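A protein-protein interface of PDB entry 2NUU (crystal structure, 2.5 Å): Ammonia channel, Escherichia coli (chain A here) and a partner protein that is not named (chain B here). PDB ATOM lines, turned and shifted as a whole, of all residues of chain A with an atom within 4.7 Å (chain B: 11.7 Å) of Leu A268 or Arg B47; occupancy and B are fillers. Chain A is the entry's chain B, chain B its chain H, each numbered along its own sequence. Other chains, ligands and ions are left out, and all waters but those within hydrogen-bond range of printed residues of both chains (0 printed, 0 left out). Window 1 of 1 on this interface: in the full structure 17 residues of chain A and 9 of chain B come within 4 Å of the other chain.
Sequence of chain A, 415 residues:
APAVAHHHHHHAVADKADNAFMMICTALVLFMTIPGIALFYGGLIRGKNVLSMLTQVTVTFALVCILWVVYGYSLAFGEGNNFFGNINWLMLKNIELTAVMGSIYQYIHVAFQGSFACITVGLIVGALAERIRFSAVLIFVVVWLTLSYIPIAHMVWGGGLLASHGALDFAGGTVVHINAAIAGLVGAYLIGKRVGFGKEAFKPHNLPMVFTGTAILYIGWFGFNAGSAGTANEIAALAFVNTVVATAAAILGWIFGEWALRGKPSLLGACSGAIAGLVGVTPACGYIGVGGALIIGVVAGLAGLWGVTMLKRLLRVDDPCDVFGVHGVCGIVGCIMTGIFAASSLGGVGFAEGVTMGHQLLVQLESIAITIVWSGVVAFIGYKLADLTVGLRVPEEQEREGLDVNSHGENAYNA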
ATOM      1  N   PHE A  40      27.551   3.972  23.407  1.00  0.00           N
ATOM      2  CA  PHE A  40      27.196   5.069  22.516  1.00  0.00           C
ATOM      3  C   PHE A  40      26.578   6.237  23.291  1.00  0.00           C
ATOM      4  O   PHE A  40      27.062   7.377  23.224  1.00  0.00           O
ATOM      5  CB  PHE A  40      26.241   4.575  21.425  1.00  0.00           C
ATOM      6  CG  PHE A  40      25.947   5.605  20.356  1.00  0.00           C
ATOM      7  CD1 PHE A  40      26.923   5.967  19.424  1.00  0.00           C
ATOM      8  CD2 PHE A  40      24.685   6.197  20.273  1.00  0.00           C
ATOM      9  CE1 PHE A  40      26.650   6.914  18.435  1.00  0.00           C
ATOM     10  CE2 PHE A  40      24.397   7.148  19.288  1.00  0.00           C
ATOM     11  CZ  PHE A  40      25.376   7.512  18.366  1.00  0.00           C
ATOM     12  N   LEU A  44      27.994  10.131  24.994  1.00  0.00           N
ATOM     13  CA  LEU A  44      27.350  11.385  24.552  1.00  0.00           C
ATOM     14  C   LEU A  44      26.949  12.309  25.686  1.00  0.00           C
ATOM     15  O   LEU A  44      26.765  13.508  25.478  1.00  0.00           O
ATOM     16  CB  LEU A  44      26.126  11.102  23.667  1.00  0.00           C
ATOM     17  CG  LEU A  44      26.416  10.630  22.241  1.00  0.00           C
ATOM     18  CD1 LEU A  44      25.166  10.129  21.571  1.00  0.00           C
ATOM     19  CD2 LEU A  44      27.057  11.738  21.421  1.00  0.00           C
ATOM     20  N   PRO A 204      29.751  15.850  24.896  1.00  0.00           N
ATOM     21  CA  PRO A 204      30.015  14.434  25.156  1.00  0.00           C
ATOM     22  C   PRO A 204      31.282  14.280  26.025  1.00  0.00           C
ATOM     23  O   PRO A 204      32.335  14.831  25.676  1.00  0.00           O
ATOM     24  CB  PRO A 204      30.253  13.857  23.754  1.00  0.00           C
ATOM     25  CG  PRO A 204      29.598  14.791  22.830  1.00  0.00           C
ATOM     26  CD  PRO A 204      29.687  16.148  23.453  1.00  0.00           C
ATOM     27  N   LEU A 207      34.340  10.996  23.662  1.00  0.00           N
ATOM     28  CA  LEU A 207      34.101  10.652  22.253  1.00  0.00           C
ATOM     29  C   LEU A 207      34.686   9.303  21.766  1.00  0.00           C
ATOM     30  O   LEU A 207      34.051   8.630  20.946  1.00  0.00           O
ATOM     31  CB  LEU A 207      34.516  11.795  21.320  1.00  0.00           C
ATOM     32  CG  LEU A 207      33.632  13.053  21.368  1.00  0.00           C
ATOM     33  CD1 LEU A 207      34.252  14.206  20.587  1.00  0.00           C
ATOM     34  CD2 LEU A 207      32.230  12.756  20.847  1.00  0.00           C
ATOM     35  N   VAL A 210      31.971   6.932  22.557  1.00  0.00           N
ATOM     36  CA  VAL A 210      30.890   7.022  21.563  1.00  0.00           C
ATOM     37  C   VAL A 210      31.261   6.188  20.324  1.00  0.00           C
ATOM     38  O   VAL A 210      30.471   5.370  19.855  1.00  0.00           O
ATOM     39  CB  VAL A 210      30.571   8.484  21.187  1.00  0.00           C
ATOM     40  CG1 VAL A 210      29.514   8.558  20.075  1.00  0.00           C
ATOM     41  CG2 VAL A 210      30.101   9.250  22.405  1.00  0.00           C
ATOM     42  N   ARG A 262      29.203  23.337   7.964  1.00  0.00           N
ATOM     43  CA  ARG A 262      29.759  23.817   9.220  1.00  0.00           C
ATOM     44  C   ARG A 262      31.261  24.129   9.168  1.00  0.00           C
ATOM     45  O   ARG A 262      31.773  24.839  10.030  1.00  0.00           O
ATOM     46  CB  ARG A 262      29.327  22.924  10.385  1.00  0.00           C
ATOM     47  CG  ARG A 262      27.880  23.230  10.808  1.00  0.00           C
ATOM     48  CD  ARG A 262      27.217  22.087  11.553  1.00  0.00           C
ATOM     49  NE  ARG A 262      27.282  22.261  13.003  1.00  0.00           N
ATOM     50  CZ  ARG A 262      26.419  22.982  13.717  1.00  0.00           C
ATOM     51  NH1 ARG A 262      25.411  23.613  13.126  1.00  0.00           N
ATOM     52  NH2 ARG A 262      26.566  23.076  15.033  1.00  0.00           N
ATOM     53  N   SER A 266      33.656  16.187  11.556  1.00  0.00           N
ATOM     54  CA  SER A 266      33.897  15.741  12.929  1.00  0.00           C
ATOM     55  C   SER A 266      33.675  14.249  13.138  1.00  0.00           C
ATOM     56  O   SER A 266      33.011  13.584  12.332  1.00  0.00           O
ATOM     57  CB  SER A 266      33.011  16.542  13.883  1.00  0.00           C
ATOM     58  OG  SER A 266      31.646  16.208  13.697  1.00  0.00           O
ATOM     59  N   LEU A 267      34.224  13.722  14.230  1.00  0.00           N
ATOM     60  CA  LEU A 267      34.059  12.300  14.526  1.00  0.00           C
ATOM     61  C   LEU A 267      32.612  11.976  14.917  1.00  0.00           C
ATOM     62  O   LEU A 267      32.087  10.917  14.545  1.00  0.00           O
ATOM     63  CB  LEU A 267      35.014  11.832  15.625  1.00  0.00           C
ATOM     64  CG  LEU A 267      34.690  10.383  16.017  1.00  0.00           C
ATOM     65  CD1 LEU A 267      35.113   9.366  14.924  1.00  0.00           C
ATOM     66  CD2 LEU A 267      35.261  10.039  17.360  1.00  0.00           C
ATOM     67  N   LEU A 268      31.975  12.886  15.663  1.00  0.00           N
ATOM     68  CA  LEU A 268      30.594  12.683  16.082  1.00  0.00           C
ATOM     69  C   LEU A 268      29.705  12.618  14.844  1.00  0.00           C
ATOM     70  O   LEU A 268      28.721  11.896  14.833  1.00  0.00           O
ATOM     71  CB  LEU A 268      30.131  13.762  17.055  1.00  0.00           C
ATOM     72  CG  LEU A 268      28.799  13.477  17.774  1.00  0.00           C
ATOM     73  CD1 LEU A 268      28.802  12.100  18.419  1.00  0.00           C
ATOM     74  CD2 LEU A 268      28.492  14.542  18.796  1.00  0.00           C
ATOM     75  N   GLY A 269      30.112  13.330  13.791  1.00  0.00           N
ATOM     76  CA  GLY A 269      29.409  13.346  12.511  1.00  0.00           C
ATOM     77  C   GLY A 269      29.574  12.036  11.744  1.00  0.00           C
ATOM     78  O   GLY A 269      28.605  11.521  11.178  1.00  0.00           O
ATOM     79  N   ALA A 270      30.788  11.489  11.726  1.00  0.00           N
ATOM     80  CA  ALA A 270      31.049  10.223  11.033  1.00  0.00           C
ATOM     81  C   ALA A 270      30.281   9.086  11.719  1.00  0.00           C
ATOM     82  O   ALA A 270      29.691   8.231  11.048  1.00  0.00           O
ATOM     83  CB  ALA A 270      32.541   9.920  10.990  1.00  0.00           C
ATOM     84  N   CYS A 271      30.273   9.102  13.053  1.00  0.00           N
ATOM     85  CA  CYS A 271      29.554   8.096  13.845  1.00  0.00           C
ATOM     86  C   CYS A 271      28.046   8.220  13.639  1.00  0.00           C
ATOM     87  O   CYS A 271      27.360   7.224  13.360  1.00  0.00           O
ATOM     88  CB  CYS A 271      29.874   8.235  15.337  1.00  0.00           C
ATOM     89  SG  CYS A 271      31.575   7.856  15.776  1.00  0.00           S
ATOM     90  N   SER A 272      27.535   9.444  13.773  1.00  0.00           N
ATOM     91  CA  SER A 272      26.106   9.690  13.603  1.00  0.00           C
ATOM     92  C   SER A 272      25.638   9.253  12.210  1.00  0.00           C
ATOM     93  O   SER A 272      24.561   8.680  12.067  1.00  0.00           O
ATOM     94  CB  SER A 272      25.780  11.149  13.876  1.00  0.00           C
ATOM     95  OG  SER A 272      25.940  11.440  15.252  1.00  0.00           O
ATOM     96  N   VAL A 308      19.374  16.245  13.712  1.00  0.00           N
ATOM     97  CA  VAL A 308      20.105  16.647  14.916  1.00  0.00           C
ATOM     98  C   VAL A 308      20.420  18.144  14.952  1.00  0.00           C
ATOM     99  O   VAL A 308      20.859  18.669  15.978  1.00  0.00           O
ATOM    100  CB  VAL A 308      21.406  15.808  15.096  1.00  0.00           C
ATOM    101  CG1 VAL A 308      21.122  14.329  14.872  1.00  0.00           C
ATOM    102  CG2 VAL A 308      22.517  16.285  14.164  1.00  0.00           C
ATOM    103  N   THR A 309      20.180  18.823  13.832  1.00  0.00           N
ATOM    104  CA  THR A 309      20.439  20.255  13.719  1.00  0.00           C
ATOM    105  C   THR A 309      19.165  21.115  13.670  1.00  0.00           C
ATOM    106  O   THR A 309      18.822  21.793  14.645  1.00  0.00           O
ATOM    107  CB  THR A 309      21.328  20.569  12.476  1.00  0.00           C
ATOM    108  OG1 THR A 309      22.525  19.793  12.536  1.00  0.00           O
ATOM    109  CG2 THR A 309      21.707  22.042  12.433  1.00  0.00           C
ATOM    110  N   CYS A 321      20.421  12.555  23.397  1.00  0.00           N
ATOM    111  CA  CYS A 321      21.102  11.709  22.425  1.00  0.00           C
ATOM    112  C   CYS A 321      20.501  11.685  21.024  1.00  0.00           C
ATOM    113  O   CYS A 321      20.820  10.805  20.232  1.00  0.00           O
ATOM    114  CB  CYS A 321      21.259  10.305  22.987  1.00  0.00           C
ATOM    115  SG  CYS A 321      22.218  10.320  24.492  1.00  0.00           S
ATOM    116  N   ASP A 322      19.657  12.669  20.719  1.00  0.00           N
ATOM    117  CA  ASP A 322      19.028  12.815  19.400  1.00  0.00           C
ATOM    118  C   ASP A 322      18.355  11.540  18.843  1.00  0.00           C
ATOM    119  O   ASP A 322      18.483  11.231  17.657  1.00  0.00           O
ATOM    120  CB  ASP A 322      20.062  13.356  18.382  1.00  0.00           C
ATOM    121  CG  ASP A 322      20.602  14.749  18.749  1.00  0.00           C
ATOM    122  OD1 ASP A 322      19.860  15.749  18.588  1.00  0.00           O
ATOM    123  OD2 ASP A 322      21.781  14.847  19.166  1.00  0.00           O
ATOM    124  N   VAL A 326      17.662  10.925  14.533  1.00  0.00           N
ATOM    125  CA  VAL A 326      18.284   9.824  13.799  1.00  0.00           C
ATOM    126  C   VAL A 326      17.293   8.679  13.545  1.00  0.00           C
ATOM    127  O   VAL A 326      16.908   8.448  12.402  1.00  0.00           O
ATOM    128  CB  VAL A 326      19.580   9.276  14.502  1.00  0.00           C
ATOM    129  CG1 VAL A 326      20.068   7.991  13.838  1.00  0.00           C
ATOM    130  CG2 VAL A 326      20.703  10.318  14.478  1.00  0.00           C
ATOM    131  N   ALA B  43      36.709  26.934  17.758  1.00  0.00           N
ATOM    132  CA  ALA B  43      35.315  26.634  17.997  1.00  0.00           C
ATOM    133  C   ALA B  43      35.147  25.121  17.888  1.00  0.00           C
ATOM    134  O   ALA B  43      35.863  24.465  17.129  1.00  0.00           O
ATOM    135  CB  ALA B  43      34.429  27.361  16.981  1.00  0.00           C
ATOM    136  N   GLU B  44      34.217  24.582  18.671  1.00  0.00           N
ATOM    137  CA  GLU B  44      33.932  23.152  18.702  1.00  0.00           C
ATOM    138  C   GLU B  44      32.513  22.869  18.215  1.00  0.00           C
ATOM    139  O   GLU B  44      31.598  23.638  18.483  1.00  0.00           O
ATOM    140  CB  GLU B  44      34.158  22.600  20.113  1.00  0.00           C
ATOM    141  CG  GLU B  44      35.557  22.905  20.667  1.00  0.00           C
ATOM    142  CD  GLU B  44      35.911  22.148  21.942  1.00  0.00           C
ATOM    143  OE1 GLU B  44      35.096  21.319  22.418  1.00  0.00           O
ATOM    144  OE2 GLU B  44      37.029  22.383  22.461  1.00  0.00           O
ATOM    145  N   LEU B  45      32.361  21.763  17.488  1.00  0.00           N
ATOM    146  CA  LEU B  45      31.091  21.330  16.902  1.00  0.00           C
ATOM    147  C   LEU B  45      30.670  19.964  17.464  1.00  0.00           C
ATOM    148  O   LEU B  45      31.452  19.015  17.444  1.00  0.00           O
ATOM    149  CB  LEU B  45      31.254  21.277  15.372  1.00  0.00           C
ATOM    150  CG  LEU B  45      30.361  20.575  14.331  1.00  0.00           C
ATOM    151  CD1 LEU B  45      30.903  20.836  12.927  1.00  0.00           C
ATOM    152  CD2 LEU B  45      30.251  19.070  14.538  1.00  0.00           C
ATOM    153  N   TYR B  46      29.439  19.871  17.970  1.00  0.00           N
ATOM    154  CA  TYR B  46      28.907  18.617  18.526  1.00  0.00           C
ATOM    155  C   TYR B  46      27.476  18.462  18.042  1.00  0.00           C
ATOM    156  O   TYR B  46      26.546  19.046  18.609  1.00  0.00           O
ATOM    157  CB  TYR B  46      29.012  18.582  20.057  1.00  0.00           C
ATOM    158  CG  TYR B  46      30.449  18.633  20.567  1.00  0.00           C
ATOM    159  CD1 TYR B  46      31.311  17.534  20.418  1.00  0.00           C
ATOM    160  CD2 TYR B  46      30.952  19.786  21.183  1.00  0.00           C
ATOM    161  CE1 TYR B  46      32.638  17.587  20.871  1.00  0.00           C
ATOM    162  CE2 TYR B  46      32.277  19.846  21.644  1.00  0.00           C
ATOM    163  CZ  TYR B  46      33.108  18.745  21.491  1.00  0.00           C
ATOM    164  OH  TYR B  46      34.404  18.802  21.953  1.00  0.00           O
ATOM    165  N   ARG B  47      27.322  17.698  16.962  1.00  0.00           N
ATOM    166  CA  ARG B  47      26.032  17.485  16.315  1.00  0.00           C
ATOM    167  C   ARG B  47      25.435  18.862  16.021  1.00  0.00           C
ATOM    168  O   ARG B  47      25.977  19.585  15.182  1.00  0.00           O
ATOM    169  CB  ARG B  47      25.126  16.560  17.134  1.00  0.00           C
ATOM    170  CG  ARG B  47      25.445  15.111  16.853  1.00  0.00           C
ATOM    171  CD  ARG B  47      24.766  14.169  17.804  1.00  0.00           C
ATOM    172  NE  ARG B  47      24.768  12.808  17.270  1.00  0.00           N
ATOM    173  CZ  ARG B  47      24.045  11.804  17.753  1.00  0.00           C
ATOM    174  NH1 ARG B  47      23.235  11.990  18.794  1.00  0.00           N
ATOM    175  NH2 ARG B  47      24.121  10.608  17.178  1.00  0.00           N
ATOM    176  N   GLY B  48      24.381  19.241  16.744  1.00  0.00           N
ATOM    177  CA  GLY B  48      23.752  20.539  16.570  1.00  0.00           C
ATOM    178  C   GLY B  48      24.390  21.652  17.403  1.00  0.00           C
ATOM    179  O   GLY B  48      24.222  22.833  17.093  1.00  0.00           O
ATOM    180  N   ALA B  49      25.122  21.292  18.459  1.00  0.00           N
ATOM    181  CA  ALA B  49      25.753  22.304  19.317  1.00  0.00           C
ATOM    182  C   ALA B  49      26.966  22.995  18.682  1.00  0.00           C
ATOM    183  O   ALA B  49      27.766  22.375  17.989  1.00  0.00           O
ATOM    184  CB  ALA B  49      26.117  21.721  20.666  1.00  0.00           C
ATOM    185  N   GLU B  50      27.090  24.285  18.950  1.00  0.00           N
ATOM    186  CA  GLU B  50      28.183  25.099  18.448  1.00  0.00           C
ATOM    187  C   GLU B  50      28.747  25.863  19.645  1.00  0.00           C
ATOM    188  O   GLU B  50      28.097  26.765  20.171  1.00  0.00           O
ATOM    189  CB  GLU B  50      27.661  26.065  17.386  1.00  0.00           C
ATOM    190  CG  GLU B  50      28.664  27.102  16.882  1.00  0.00           C
ATOM    191  CD  GLU B  50      29.486  26.628  15.692  1.00  0.00           C
ATOM    192  OE1 GLU B  50      29.161  25.569  15.107  1.00  0.00           O
ATOM    193  OE2 GLU B  50      30.458  27.333  15.341  1.00  0.00           O
ATOM    194  N   TYR B  51      29.939  25.480  20.095  1.00  0.00           N
ATOM    195  CA  TYR B  51      30.560  26.154  21.233  1.00  0.00           C
ATOM    196  C   TYR B  51      31.736  27.015  20.758  1.00  0.00           C
ATOM    197  O   TYR B  51      32.774  26.498  20.333  1.00  0.00           O
ATOM    198  CB  TYR B  51      30.969  25.147  22.302  1.00  0.00           C
ATOM    199  CG  TYR B  51      29.824  24.321  22.859  1.00  0.00           C
ATOM    200  CD1 TYR B  51      28.905  24.867  23.752  1.00  0.00           C
ATOM    201  CD2 TYR B  51      29.679  22.987  22.510  1.00  0.00           C
ATOM    202  CE1 TYR B  51      27.860  24.091  24.270  1.00  0.00           C
ATOM    203  CE2 TYR B  51      28.648  22.207  23.017  1.00  0.00           C
ATOM    204  CZ  TYR B  51      27.745  22.756  23.896  1.00  0.00           C
ATOM    205  OH  TYR B  51      26.727  21.961  24.387  1.00  0.00           O
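The backbone carbonyl oxygen (O) of Gly B48 lies within hydrogen-bond range of the guanidinium group (NH2) of Arg A262 (3.1 Å). OD2 of Asp A322 is in salt-bridge range of NH1 of Arg B47 (3.2 Å). The side-chain hydroxyl (OG) of Ser A272 is in hydrogen-bond range of the guanidinium group (NE) of Arg B47, at 2.7 Å. NH2 of Arg A262 lies within hydrogen-bond range of O of Ala B49 (3.3 Å). OE1 of Glu B50 lies within salt-bridge range of NH2 of Arg A262 (3.6 Å). O of Cys A321 sits at hydrogen-bond distance from NH1 of Arg B47, 3.1 Å away.
The backbone carbonyl oxygen of Leu A268 sits at hydrogen-bond distance from the side-chain hydroxyl of Ser A272 (2.8 Å). OG of Ser A266 is in hydrogen-bond range of N of Gly A269 (3.3 Å). OE1 of Glu B44 sits at hydrogen-bond distance from OH of Tyr B46 (2.7 Å).
Among the printed residues, merely in contact across the chains: Phe A40 with Arg B47 (3.5 Å), Leu A44 with Arg B47 (3.9 Å), Pro A204 with Tyr B46 (3.7 Å), Leu A207 with Tyr B46 (3.8 Å), Arg A262 with Leu B45 (3.6 Å), Arg A262 with Arg B47 (3.5 Å), Ser A266 with Leu B45 (3.3 Å), Leu A268 with Arg B47 (3.7 Å), Val A308 with Arg B47 (3.96 Å) and Val A308 with Gly B48 (3.5 Å).
Of the printed residues of chain B, Pro A204 touches Tyr B46 (3.7 Å). No residue of chain B comes within 4 Å of Val A210. Of chain B, only Leu B45 (3.3 Å) comes within 4 Å of Ser A266. Leu A267 touches none of the printed residues of chain B. Leu A268 touches just one residue of chain B: Arg B47 (3.7 Å). Gly A269 touches none of the printed residues of chain B. No residue of chain B comes within 4 Å of Cys A271. Ser A272 touches just one residue of chain B: Arg B47 (2.7 Å). Of chain B, only Arg B47 (3.96 Å) and Gly B48 (3.5 Å) come within 4 Å of Val A308. Of chain B, only Arg B47 comes within 4 Å of Cys A321. Asp A322 touches just one residue of chain B: Arg B47 (3.2 Å). Glu B44 touches none of the printed residues of chain A. Of chain A, only Phe A40, Leu A44, Arg A262, Leu A268, Ser A272, Val A308, Cys A321 and Asp A322 come within 4 Å of Arg B47. Of the printed residues of chain A, Ala B49 touches Arg A262 (3.3 Å). Tyr B51 touches none of the printed residues of chain A. The nearest residue of chain B that does not touch Leu A268 is Tyr B46 (4.1 Å).
Of the 18 printed residues of chain A, 11 touch a printed residue of chain B. Among the printed residues, 16 pairs touch across the chains.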
